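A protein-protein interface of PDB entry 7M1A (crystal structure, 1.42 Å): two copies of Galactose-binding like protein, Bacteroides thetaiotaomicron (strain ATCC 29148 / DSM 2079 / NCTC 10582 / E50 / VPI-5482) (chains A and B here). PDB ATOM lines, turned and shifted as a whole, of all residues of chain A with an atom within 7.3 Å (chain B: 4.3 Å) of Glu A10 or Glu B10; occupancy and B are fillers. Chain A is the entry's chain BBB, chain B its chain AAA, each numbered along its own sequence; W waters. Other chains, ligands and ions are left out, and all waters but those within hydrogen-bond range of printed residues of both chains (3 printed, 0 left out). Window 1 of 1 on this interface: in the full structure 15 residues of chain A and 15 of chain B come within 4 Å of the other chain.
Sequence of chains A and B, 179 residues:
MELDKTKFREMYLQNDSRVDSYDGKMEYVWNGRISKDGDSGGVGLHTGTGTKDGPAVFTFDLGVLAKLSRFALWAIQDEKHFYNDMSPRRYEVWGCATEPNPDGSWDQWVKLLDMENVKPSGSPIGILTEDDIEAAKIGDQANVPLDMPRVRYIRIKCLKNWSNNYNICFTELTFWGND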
ATOM      1  N   LYS A   7     -33.790  -9.617 -22.276  1.00  0.00           N
ATOM      2  CA  LYS A   7     -32.730  -9.113 -23.126  1.00  0.00           C
ATOM      3  C   LYS A   7     -31.340  -9.209 -22.490  1.00  0.00           C
ATOM      4  O   LYS A   7     -30.316  -8.941 -23.138  1.00  0.00           O
ATOM      5  CB  LYS A   7     -32.978  -7.671 -23.568  1.00  0.00           C
ATOM      6  CG  LYS A   7     -34.310  -7.451 -24.251  1.00  0.00           C
ATOM      7  CD  LYS A   7     -34.469  -6.074 -24.793  1.00  0.00           C
ATOM      8  CE  LYS A   7     -35.829  -5.952 -25.487  1.00  0.00           C
ATOM      9  NZ  LYS A   7     -36.061  -7.077 -26.466  1.00  0.00           N
ATOM     10  N   PHE A   8     -31.261  -9.533 -21.184  1.00  0.00           N
ATOM     11  CA  PHE A   8     -29.950  -9.534 -20.508  1.00  0.00           C
ATOM     12  C   PHE A   8     -29.138 -10.715 -21.087  1.00  0.00           C
ATOM     13  O   PHE A   8     -29.664 -11.801 -21.450  1.00  0.00           O
ATOM     14  CB  PHE A   8     -30.102  -9.759 -18.998  1.00  0.00           C
ATOM     15  CG  PHE A   8     -30.626  -8.600 -18.193  1.00  0.00           C
ATOM     16  CD1 PHE A   8     -31.236  -7.452 -18.784  1.00  0.00           C
ATOM     17  CD2 PHE A   8     -30.446  -8.650 -16.809  1.00  0.00           C
ATOM     18  CE1 PHE A   8     -31.765  -6.451 -17.964  1.00  0.00           C
ATOM     19  CE2 PHE A   8     -30.955  -7.625 -15.999  1.00  0.00           C
ATOM     20  CZ  PHE A   8     -31.620  -6.554 -16.577  1.00  0.00           C
ATOM     21  N   ARG A   9     -27.813 -10.559 -21.145  1.00  0.00           N
ATOM     22  CA  ARG A   9     -26.960 -11.625 -21.678  1.00  0.00           C
ATOM     23  C   ARG A   9     -25.699 -11.732 -20.831  1.00  0.00           C
ATOM     24  O   ARG A   9     -25.089 -10.716 -20.452  1.00  0.00           O
ATOM     25  CB  ARG A   9     -26.494 -11.393 -23.124  1.00  0.00           C
ATOM     26  CG  ARG A   9     -27.634 -11.263 -24.113  1.00  0.00           C
ATOM     27  CD  ARG A   9     -28.278 -12.638 -24.391  1.00  0.00           C
ATOM     28  NE  ARG A   9     -29.303 -12.552 -25.404  1.00  0.00           N
ATOM     29  CZ  ARG A   9     -30.614 -12.443 -25.185  1.00  0.00           C
ATOM     30  NH1 ARG A   9     -31.080 -12.447 -23.958  1.00  0.00           N
ATOM     31  NH2 ARG A   9     -31.429 -12.342 -26.225  1.00  0.00           N
ATOM     32  N   GLU A  10     -25.331 -12.991 -20.497  1.00  0.00           N
ATOM     33  CA  GLU A  10     -24.035 -13.267 -19.877  1.00  0.00           C
ATOM     34  C   GLU A  10     -22.893 -12.827 -20.792  1.00  0.00           C
ATOM     35  O   GLU A  10     -23.023 -12.839 -22.007  1.00  0.00           O
ATOM     36  CB  GLU A  10     -24.007 -14.784 -19.592  1.00  0.00           C
ATOM     37  CG  GLU A  10     -22.734 -15.313 -18.880  1.00  0.00           C
ATOM     38  CD  GLU A  10     -21.634 -15.843 -19.788  1.00  0.00           C
ATOM     39  OE1 GLU A  10     -21.628 -15.412 -20.972  1.00  0.00           O
ATOM     40  OE2 GLU A  10     -20.734 -16.449 -19.241  1.00  0.00           O
ATOM     41  N   MET A  11     -21.809 -12.342 -20.172  1.00  0.00           N
ATOM     42  CA  MET A  11     -20.558 -12.121 -20.904  1.00  0.00           C
ATOM     43  C   MET A  11     -19.464 -12.815 -20.086  1.00  0.00           C
ATOM     44  O   MET A  11     -19.653 -13.203 -18.931  1.00  0.00           O
ATOM     45  CB  MET A  11     -20.248 -10.625 -20.999  1.00  0.00           C
ATOM     46  CG  MET A  11     -21.289  -9.985 -21.870  1.00  0.00           C
ATOM     47  SD  MET A  11     -20.904  -8.077 -22.199  1.00  0.00           S
ATOM     48  CE  MET A  11     -19.459  -8.387 -23.470  1.00  0.00           C
ATOM     49  N   TYR A  12     -18.286 -12.895 -20.668  1.00  0.00           N
ATOM     50  CA  TYR A  12     -17.169 -13.555 -20.013  1.00  0.00           C
ATOM     51  C   TYR A  12     -15.904 -12.893 -20.534  1.00  0.00           C
ATOM     52  O   TYR A  12     -15.518 -13.169 -21.688  1.00  0.00           O
ATOM     53  CB  TYR A  12     -17.125 -15.070 -20.196  1.00  0.00           C
ATOM     54  CG  TYR A  12     -16.080 -15.665 -19.267  1.00  0.00           C
ATOM     55  CD1 TYR A  12     -16.294 -15.790 -17.883  1.00  0.00           C
ATOM     56  CD2 TYR A  12     -14.801 -15.965 -19.748  1.00  0.00           C
ATOM     57  CE1 TYR A  12     -15.273 -16.189 -17.001  1.00  0.00           C
ATOM     58  CE2 TYR A  12     -13.838 -16.486 -18.910  1.00  0.00           C
ATOM     59  CZ  TYR A  12     -14.043 -16.519 -17.543  1.00  0.00           C
ATOM     60  OH  TYR A  12     -13.046 -16.810 -16.674  1.00  0.00           O
ATOM     61  N   LEU A  13     -15.354 -11.985 -19.703  1.00  0.00           N
ATOM     62  CA  LEU A  13     -14.097 -11.346 -20.067  1.00  0.00           C
ATOM     63  C   LEU A  13     -12.908 -12.017 -19.394  1.00  0.00           C
ATOM     64  O   LEU A  13     -13.076 -12.696 -18.398  1.00  0.00           O
ATOM     65  CB  LEU A  13     -14.205  -9.907 -19.561  1.00  0.00           C
ATOM     66  CG  LEU A  13     -15.447  -9.090 -19.951  1.00  0.00           C
ATOM     67  CD1 LEU A  13     -15.326  -7.591 -19.593  1.00  0.00           C
ATOM     68  CD2 LEU A  13     -15.720  -9.209 -21.448  1.00  0.00           C
ATOM     69  N   ASP A  16     -12.465 -12.934 -15.553  1.00  0.00           N
ATOM     70  CA  ASP A  16     -13.695 -12.976 -14.765  1.00  0.00           C
ATOM     71  C   ASP A  16     -13.798 -14.272 -13.990  1.00  0.00           C
ATOM     72  O   ASP A  16     -13.292 -15.334 -14.408  1.00  0.00           O
ATOM     73  CB  ASP A  16     -14.921 -12.876 -15.693  1.00  0.00           C
ATOM     74  CG  ASP A  16     -15.195 -11.454 -16.221  1.00  0.00           C
ATOM     75  OD1 ASP A  16     -14.533 -10.492 -15.754  1.00  0.00           O
ATOM     76  OD2 ASP A  16     -16.164 -11.273 -16.955  1.00  0.00           O
ATOM     77  N   SER A  17     -14.550 -14.239 -12.876  1.00  0.00           N
ATOM     78  CA  SER A  17     -14.810 -15.439 -12.094  1.00  0.00           C
ATOM     79  C   SER A  17     -15.848 -16.287 -12.840  1.00  0.00           C
ATOM     80  O   SER A  17     -16.853 -15.753 -13.301  1.00  0.00           O
ATOM     81  CB  SER A  17     -15.425 -15.080 -10.758  1.00  0.00           C
ATOM     82  OG  SER A  17     -14.487 -14.285 -10.056  1.00  0.00           O
ATOM     83  N   VAL A  19     -19.081 -18.602 -12.471  1.00  0.00           N
ATOM     84  CA  VAL A  19     -20.214 -18.407 -11.546  1.00  0.00           C
ATOM     85  C   VAL A  19     -21.114 -19.647 -11.501  1.00  0.00           C
ATOM     86  O   VAL A  19     -22.304 -19.550 -11.126  1.00  0.00           O
ATOM     87  CB  VAL A  19     -21.018 -17.096 -11.761  1.00  0.00           C
ATOM     88  CG1 VAL A  19     -20.085 -15.847 -11.605  1.00  0.00           C
ATOM     89  CG2 VAL A  19     -21.659 -17.082 -13.151  1.00  0.00           C
ATOM     90  N   ASP A  20     -20.572 -20.817 -11.878  1.00  0.00           N
ATOM     91  CA  ASP A  20     -21.419 -21.982 -12.178  1.00  0.00           C
ATOM     92  C   ASP A  20     -21.184 -23.100 -11.143  1.00  0.00           C
ATOM     93  O   ASP A  20     -21.487 -24.236 -11.390  1.00  0.00           O
ATOM     94  CB  ASP A  20     -21.131 -22.489 -13.609  1.00  0.00           C
ATOM     95  CG  ASP A  20     -21.508 -21.448 -14.658  1.00  0.00           C
ATOM     96  OD1 ASP A  20     -22.238 -20.437 -14.367  1.00  0.00           O
ATOM     97  OD2 ASP A  20     -20.956 -21.547 -15.742  1.00  0.00           O
ATOM     98  N   LYS A  25     -25.724 -20.688 -12.507  1.00  0.00           N
ATOM     99  CA  LYS A  25     -25.618 -20.141 -13.852  1.00  0.00           C
ATOM    100  C   LYS A  25     -25.908 -18.665 -13.755  1.00  0.00           C
ATOM    101  O   LYS A  25     -26.837 -18.253 -13.046  1.00  0.00           O
ATOM    102  CB  LYS A  25     -26.568 -20.842 -14.847  1.00  0.00           C
ATOM    103  CG  LYS A  25     -26.136 -20.587 -16.269  1.00  0.00           C
ATOM    104  CD  LYS A  25     -24.853 -21.353 -16.711  1.00  0.00           C
ATOM    105  CE  LYS A  25     -24.513 -20.996 -18.165  1.00  0.00           C
ATOM    106  NZ  LYS A  25     -24.177 -19.530 -18.351  1.00  0.00           N
ATOM    107  N   MET A  26     -25.193 -17.824 -14.518  1.00  0.00           N
ATOM    108  CA  MET A  26     -25.466 -16.388 -14.391  1.00  0.00           C
ATOM    109  C   MET A  26     -26.907 -16.044 -14.782  1.00  0.00           C
ATOM    110  O   MET A  26     -27.494 -15.190 -14.125  1.00  0.00           O
ATOM    111  CB  MET A  26     -24.517 -15.575 -15.292  1.00  0.00           C
ATOM    112  CG  MET A  26     -24.564 -14.138 -14.782  1.00  0.00           C
ATOM    113  SD  MET A  26     -23.406 -12.946 -15.952  1.00  0.00           S
ATOM    114  CE  MET A  26     -21.667 -13.803 -15.610  1.00  0.00           C
ATOM    115  N   GLU A  27     -27.498 -16.732 -15.811  1.00  0.00           N
ATOM    116  CA  GLU A  27     -28.842 -16.392 -16.243  1.00  0.00           C
ATOM    117  C   GLU A  27     -29.840 -16.611 -15.110  1.00  0.00           C
ATOM    118  O   GLU A  27     -30.906 -16.031 -15.150  1.00  0.00           O
ATOM    119  CB  GLU A  27     -29.227 -17.239 -17.456  1.00  0.00           C
ATOM    120  CG  GLU A  27     -28.446 -16.883 -18.719  1.00  0.00           C
ATOM    121  CD  GLU A  27     -27.055 -17.429 -18.965  1.00  0.00           C
ATOM    122  OE1 GLU A  27     -26.484 -18.070 -18.075  1.00  0.00           O
ATOM    123  OE2 GLU A  27     -26.619 -17.248 -20.135  1.00  0.00           O
ATOM    124  N   TRP A  30     -31.309 -13.397 -13.403  1.00  0.00           N
ATOM    125  CA  TRP A  30     -32.281 -12.526 -14.066  1.00  0.00           C
ATOM    126  C   TRP A  30     -33.442 -13.333 -14.620  1.00  0.00           C
ATOM    127  O   TRP A  30     -34.020 -12.907 -15.586  1.00  0.00           O
ATOM    128  CB  TRP A  30     -31.607 -11.563 -15.051  1.00  0.00           C
ATOM    129  CG  TRP A  30     -30.823 -12.243 -16.147  1.00  0.00           C
ATOM    130  CD1 TRP A  30     -31.344 -12.855 -17.247  1.00  0.00           C
ATOM    131  CD2 TRP A  30     -29.390 -12.221 -16.349  1.00  0.00           C
ATOM    132  NE1 TRP A  30     -30.340 -13.320 -18.095  1.00  0.00           N
ATOM    133  CE2 TRP A  30     -29.132 -12.862 -17.600  1.00  0.00           C
ATOM    134  CE3 TRP A  30     -28.341 -11.673 -15.612  1.00  0.00           C
ATOM    135  CZ2 TRP A  30     -27.843 -13.003 -18.083  1.00  0.00           C
ATOM    136  CZ3 TRP A  30     -27.091 -11.776 -16.121  1.00  0.00           C
ATOM    137  CH2 TRP A  30     -26.829 -12.398 -17.353  1.00  0.00           C
ATOM    138  N   THR A  59     -19.476 -10.190 -15.444  1.00  0.00           N
ATOM    139  CA  THR A  59     -19.843  -9.184 -16.420  1.00  0.00           C
ATOM    140  C   THR A  59     -21.096  -9.647 -17.170  1.00  0.00           C
ATOM    141  O   THR A  59     -21.261 -10.827 -17.534  1.00  0.00           O
ATOM    142  CB  THR A  59     -18.710  -9.030 -17.437  1.00  0.00           C
ATOM    143  OG1 THR A  59     -17.441  -8.850 -16.738  1.00  0.00           O
ATOM    144  CG2 THR A  59     -18.920  -7.872 -18.395  1.00  0.00           C
ATOM    145  N   PHE A  60     -21.960  -8.666 -17.471  1.00  0.00           N
ATOM    146  CA  PHE A  60     -23.164  -8.966 -18.266  1.00  0.00           C
ATOM    147  C   PHE A  60     -23.611  -7.748 -19.053  1.00  0.00           C
ATOM    148  O   PHE A  60     -23.091  -6.635 -18.891  1.00  0.00           O
ATOM    149  CB  PHE A  60     -24.308  -9.633 -17.489  1.00  0.00           C
ATOM    150  CG  PHE A  60     -24.795  -8.821 -16.338  1.00  0.00           C
ATOM    151  CD1 PHE A  60     -24.141  -8.831 -15.115  1.00  0.00           C
ATOM    152  CD2 PHE A  60     -26.000  -8.073 -16.436  1.00  0.00           C
ATOM    153  CE1 PHE A  60     -24.650  -8.113 -14.006  1.00  0.00           C
ATOM    154  CE2 PHE A  60     -26.458  -7.358 -15.330  1.00  0.00           C
ATOM    155  CZ  PHE A  60     -25.818  -7.407 -14.114  1.00  0.00           C
ATOM    156  N   ASP A  61     -24.594  -7.978 -19.954  1.00  0.00           N
ATOM    157  CA  ASP A  61     -25.071  -7.020 -20.943  1.00  0.00           C
ATOM    158  C   ASP A  61     -26.556  -6.865 -20.656  1.00  0.00           C
ATOM    159  O   ASP A  61     -27.315  -7.839 -20.644  1.00  0.00           O
ATOM    160  CB  ASP A  61     -24.851  -7.649 -22.326  1.00  0.00           C
ATOM    161  CG  ASP A  61     -25.183  -6.769 -23.519  1.00  0.00           C
ATOM    162  OD1 ASP A  61     -25.876  -5.755 -23.398  1.00  0.00           O
ATOM    163  OD2 ASP A  61     -24.784  -7.161 -24.632  1.00  0.00           O
ATOM    164  N   ARG B   9     -23.344 -13.319 -28.132  1.00  0.00           N
ATOM    165  CA  ARG B   9     -23.538 -13.515 -26.708  1.00  0.00           C
ATOM    166  C   ARG B   9     -23.984 -14.930 -26.396  1.00  0.00           C
ATOM    167  O   ARG B   9     -24.843 -15.494 -27.114  1.00  0.00           O
ATOM    168  CB  ARG B   9     -24.628 -12.576 -26.157  1.00  0.00           C
ATOM    169  CG  ARG B   9     -24.244 -11.114 -26.287  1.00  0.00           C
ATOM    170  CD  ARG B   9     -23.205 -10.618 -25.303  1.00  0.00           C
ATOM    171  NE  ARG B   9     -22.960  -9.230 -25.389  1.00  0.00           N
ATOM    172  CZ  ARG B   9     -21.997  -8.657 -26.110  1.00  0.00           C
ATOM    173  NH1 ARG B   9     -21.186  -9.378 -26.844  1.00  0.00           N
ATOM    174  NH2 ARG B   9     -21.843  -7.351 -26.099  1.00  0.00           N
ATOM    175  N   GLU B  10     -23.394 -15.536 -25.357  1.00  0.00           N
ATOM    176  CA  GLU B  10     -23.854 -16.829 -24.858  1.00  0.00           C
ATOM    177  C   GLU B  10     -25.301 -16.689 -24.359  1.00  0.00           C
ATOM    178  O   GLU B  10     -25.697 -15.637 -23.866  1.00  0.00           O
ATOM    179  CB  GLU B  10     -22.883 -17.251 -23.750  1.00  0.00           C
ATOM    180  CG  GLU B  10     -23.157 -18.566 -23.082  1.00  0.00           C
ATOM    181  CD  GLU B  10     -24.013 -18.570 -21.851  1.00  0.00           C
ATOM    182  OE1 GLU B  10     -24.784 -17.582 -21.701  1.00  0.00           O
ATOM    183  OE2 GLU B  10     -24.034 -19.589 -21.190  1.00  0.00           O
ATOM    184  N   MET B  11     -26.081 -17.766 -24.558  1.00  0.00           N
ATOM    185  CA  MET B  11     -27.377 -17.912 -23.914  1.00  0.00           C
ATOM    186  C   MET B  11     -27.398 -19.240 -23.184  1.00  0.00           C
ATOM    187  O   MET B  11     -26.562 -20.124 -23.455  1.00  0.00           O
ATOM    188  CB  MET B  11     -28.479 -17.814 -24.938  1.00  0.00           C
ATOM    189  CG  MET B  11     -28.512 -16.449 -25.590  1.00  0.00           C
ATOM    190  SD  MET B  11     -30.042 -16.221 -26.783  1.00  0.00           S
ATOM    191  CE  MET B  11     -31.401 -16.084 -25.417  1.00  0.00           C
ATOM    192  N   TYR B  12     -28.463 -19.474 -22.378  1.00  0.00           N
ATOM    193  CA  TYR B  12     -28.516 -20.746 -21.665  1.00  0.00           C
ATOM    194  C   TYR B  12     -29.995 -20.996 -21.428  1.00  0.00           C
ATOM    195  O   TYR B  12     -30.625 -20.297 -20.611  1.00  0.00           O
ATOM    196  CB  TYR B  12     -27.776 -20.752 -20.331  1.00  0.00           C
ATOM    197  CG  TYR B  12     -27.744 -22.168 -19.788  1.00  0.00           C
ATOM    198  CD1 TYR B  12     -26.919 -23.177 -20.359  1.00  0.00           C
ATOM    199  CD2 TYR B  12     -28.665 -22.539 -18.785  1.00  0.00           C
ATOM    200  CE1 TYR B  12     -26.984 -24.490 -19.898  1.00  0.00           C
ATOM    201  CE2 TYR B  12     -28.709 -23.850 -18.320  1.00  0.00           C
ATOM    202  CZ  TYR B  12     -27.905 -24.820 -18.909  1.00  0.00           C
ATOM    203  OH  TYR B  12     -28.008 -26.103 -18.496  1.00  0.00           O
ATOM    204  N   LYS B  25     -15.296 -22.514 -22.581  1.00  0.00           N
ATOM    205  CA  LYS B  25     -16.291 -21.455 -22.419  1.00  0.00           C
ATOM    206  C   LYS B  25     -16.834 -21.162 -23.800  1.00  0.00           C
ATOM    207  O   LYS B  25     -16.155 -21.216 -24.829  1.00  0.00           O
ATOM    208  CB  LYS B  25     -15.627 -20.133 -21.936  1.00  0.00           C
ATOM    209  CG  LYS B  25     -16.683 -19.236 -21.312  1.00  0.00           C
ATOM    210  CD  LYS B  25     -17.185 -19.676 -19.960  1.00  0.00           C
ATOM    211  CE  LYS B  25     -18.350 -18.745 -19.534  1.00  0.00           C
ATOM    212  NZ  LYS B  25     -19.497 -18.634 -20.518  1.00  0.00           N
ATOM    213  N   MET B  26     -18.145 -20.901 -23.870  1.00  0.00           N
ATOM    214  CA  MET B  26     -18.786 -20.724 -25.154  1.00  0.00           C
ATOM    215  C   MET B  26     -18.103 -19.580 -25.927  1.00  0.00           C
ATOM    216  O   MET B  26     -17.936 -19.669 -27.145  1.00  0.00           O
ATOM    217  CB  MET B  26     -20.309 -20.482 -25.049  1.00  0.00           C
ATOM    218  CG  MET B  26     -20.930 -20.716 -26.491  1.00  0.00           C
ATOM    219  SD  MET B  26     -22.861 -20.360 -26.488  1.00  0.00           S
ATOM    220  CE  MET B  26     -23.416 -21.748 -25.177  1.00  0.00           C
ATOM    221  N   GLU B  27     -17.751 -18.460 -25.201  1.00  0.00           N
ATOM    222  CA  GLU B  27     -17.215 -17.289 -25.883  1.00  0.00           C
ATOM    223  C   GLU B  27     -15.905 -17.640 -26.590  1.00  0.00           C
ATOM    224  O   GLU B  27     -15.488 -16.903 -27.452  1.00  0.00           O
ATOM    225  CB  GLU B  27     -16.937 -16.200 -24.834  1.00  0.00           C
ATOM    226  CG  GLU B  27     -18.195 -15.514 -24.240  1.00  0.00           C
ATOM    227  CD  GLU B  27     -18.941 -16.238 -23.160  1.00  0.00           C
ATOM    228  OE1 GLU B  27     -18.600 -17.390 -22.751  1.00  0.00           O
ATOM    229  OE2 GLU B  27     -19.885 -15.552 -22.622  1.00  0.00           O
ATOM    230  N   TRP B  30     -16.023 -17.864 -30.484  1.00  0.00           N
ATOM    231  CA  TRP B  30     -16.104 -16.677 -31.332  1.00  0.00           C
ATOM    232  C   TRP B  30     -15.059 -15.625 -30.936  1.00  0.00           C
ATOM    233  O   TRP B  30     -15.312 -14.461 -31.115  1.00  0.00           O
ATOM    234  CB  TRP B  30     -17.553 -16.155 -31.430  1.00  0.00           C
ATOM    235  CG  TRP B  30     -18.138 -15.774 -30.103  1.00  0.00           C
ATOM    236  CD1 TRP B  30     -17.871 -14.652 -29.378  1.00  0.00           C
ATOM    237  CD2 TRP B  30     -19.240 -16.454 -29.456  1.00  0.00           C
ATOM    238  NE1 TRP B  30     -18.690 -14.610 -28.248  1.00  0.00           N
ATOM    239  CE2 TRP B  30     -19.573 -15.689 -28.278  1.00  0.00           C
ATOM    240  CE3 TRP B  30     -19.991 -17.622 -29.743  1.00  0.00           C
ATOM    241  CZ2 TRP B  30     -20.591 -16.032 -27.410  1.00  0.00           C
ATOM    242  CZ3 TRP B  30     -21.026 -17.931 -28.883  1.00  0.00           C
ATOM    243  CH2 TRP B  30     -21.332 -17.145 -27.772  1.00  0.00           C
ATOM    244  N   THR B  59     -26.914 -22.727 -27.211  1.00  0.00           N
ATOM    245  CA  THR B  59     -27.663 -21.632 -27.801  1.00  0.00           C
ATOM    246  C   THR B  59     -26.833 -20.348 -27.670  1.00  0.00           C
ATOM    247  O   THR B  59     -26.236 -20.074 -26.616  1.00  0.00           O
ATOM    248  CB  THR B  59     -28.961 -21.459 -27.023  1.00  0.00           C
ATOM    249  OG1 THR B  59     -29.696 -22.694 -26.944  1.00  0.00           O
ATOM    250  CG2 THR B  59     -29.872 -20.422 -27.643  1.00  0.00           C
HETATM  251  O   HOH W   1     -27.118 -15.028 -21.615  1.00  0.00           O
HETATM  252  O   HOH W   2     -21.478 -13.785 -24.020  1.00  0.00           O
HETATM  253  O   HOH W   3     -21.059 -20.515 -18.348  1.00  0.00           O
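NE of Arg B9 is in salt-bridge range of OD2 of Asp A61, at 2.9 Å. NZ of Lys A25 is in salt-bridge range of OE2 of Glu B10, at 2.8 Å. The side-chain carboxylate of Glu A27 sits close to the side-chain carboxylate of Glu B10, 2.4 Å away. The side-chain amino group (NZ) of Lys B25 lies within salt-bridge range of the side-chain carboxylate (OE2) of Glu A10 (2.8 Å). OE1 of Glu A10 sits close to OE2 of Glu B27, at 2.4 Å.
The backbone NH (N) of Met B11 sits at hydrogen-bond distance from the backbone carbonyl oxygen (O) of Thr B59 (3.1 Å). The side-chain amino group of Lys B25 lies within salt-bridge range of the side-chain carboxylate of Glu B27. The backbone NH (N) of Arg A9 is in hydrogen-bond range of the backbone carbonyl oxygen (O) of Asp A61 (2.8 Å). The backbone NH (N) of Met A11 is in hydrogen-bond range of the backbone carbonyl oxygen (O) of Thr A59, at 3.1 Å. The backbone carbonyl oxygen (O) of Asp A16 lies within hydrogen-bond range of the side-chain hydroxyl (OH) of Tyr A12 (2.7 Å). The side-chain amino group of Lys A25 lies within salt-bridge range of the side-chain carboxylate of Glu A27.
Among the printed residues, merely in contact across the chains: Glu A10 with Glu B10, Glu A27 with Tyr B12, Tyr A12 with Glu B27, Met A11 with Arg B9, Glu A27 with Met B11, Arg A9 with Met B11, Arg A9 with Arg B9, Met A11 with Glu B27, Lys A25 with Tyr B12, Tyr A12 with Lys B25, Glu A10 with Arg B9 and Arg A9 with Glu B10.
Of the printed residues of chain B, Glu A10 touches Arg B9 (3.98 Å), Glu B10 (3.6 Å), Lys B25 (2.8 Å) and Glu B27 (2.4 Å). Of the printed residues of chain B, Glu A27 touches Glu B10, Met B11 and Tyr B12. Printed residues of chain A within 4 Å of Glu B27: Glu A10, Met A11 and Tyr A12. Printed residues of chain B within 4 Å of Tyr A12: Lys B25 and Glu B27. Of the printed residues of chain A, Lys B25 touches Glu A10 and Tyr A12. The nearest printed residue of chain B that does not touch Glu A10 is Met B11 (6.2 Å). The nearest printed residue of chain A that does not touch Glu B10 is Phe A8 (6.0 Å). The nearest printed residue of chain B that does not touch Glu A27 is Thr B59 (7.1 Å).
Printed residues of chain B that touch a printed residue of chain A: Arg B9, Glu B10, Met B11, Tyr B12, Lys B25 and Glu B27. Along chain B the printed residues that touch a printed residue of chain A span positions 9 to 27. Hydrophobic or aromatic side chains of chain A within 4 Å of the printed part of chain B: Met A11 and Tyr A12. Among the printed residues, Asp or Glu carboxylates within 4 Å of a Lys or Arg side-chain nitrogen of the other chain: Glu A10 with Lys B25, Lys A25 with Glu B10 and Asp A61 with Arg B9.
Arg B9 touches its own counterpart, Arg A9. Glu A10 touches Glu B27, and with the chains exchanged Glu A27 touches Glu B10. Tyr A12 touches Lys B25, and with the chains exchanged Lys A25 touches Tyr B12. Tyr A12 touches Glu B27, and with the chains exchanged Glu A27 touches Tyr B12. Positions printed for both chains: 9, 10, 11, 12, 25, 26, 27, 30 and 59. Of the 17 pairs that touch across the chains among the printed residues, 16 have their exchanged pair printed and touching as well.
Water W2 lies within hydrogen-bond range of the backbone carbonyl oxygen (O) of Glu A10 (2.7 Å), the side-chain carboxylate (OE2) of Glu B27 (2.8 Å) and the backbone NH (N) of Glu B10 (2.9 Å). Water W1 lies within hydrogen-bond range of OE2 of Glu A27 (2.7 Å), O of Glu B10 (2.7 Å) and N of Glu A10 (2.9 Å). Water W3 lies within hydrogen-bond range of OD2 of Asp A20, NZ of Lys B25 and NZ of Lys A25.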
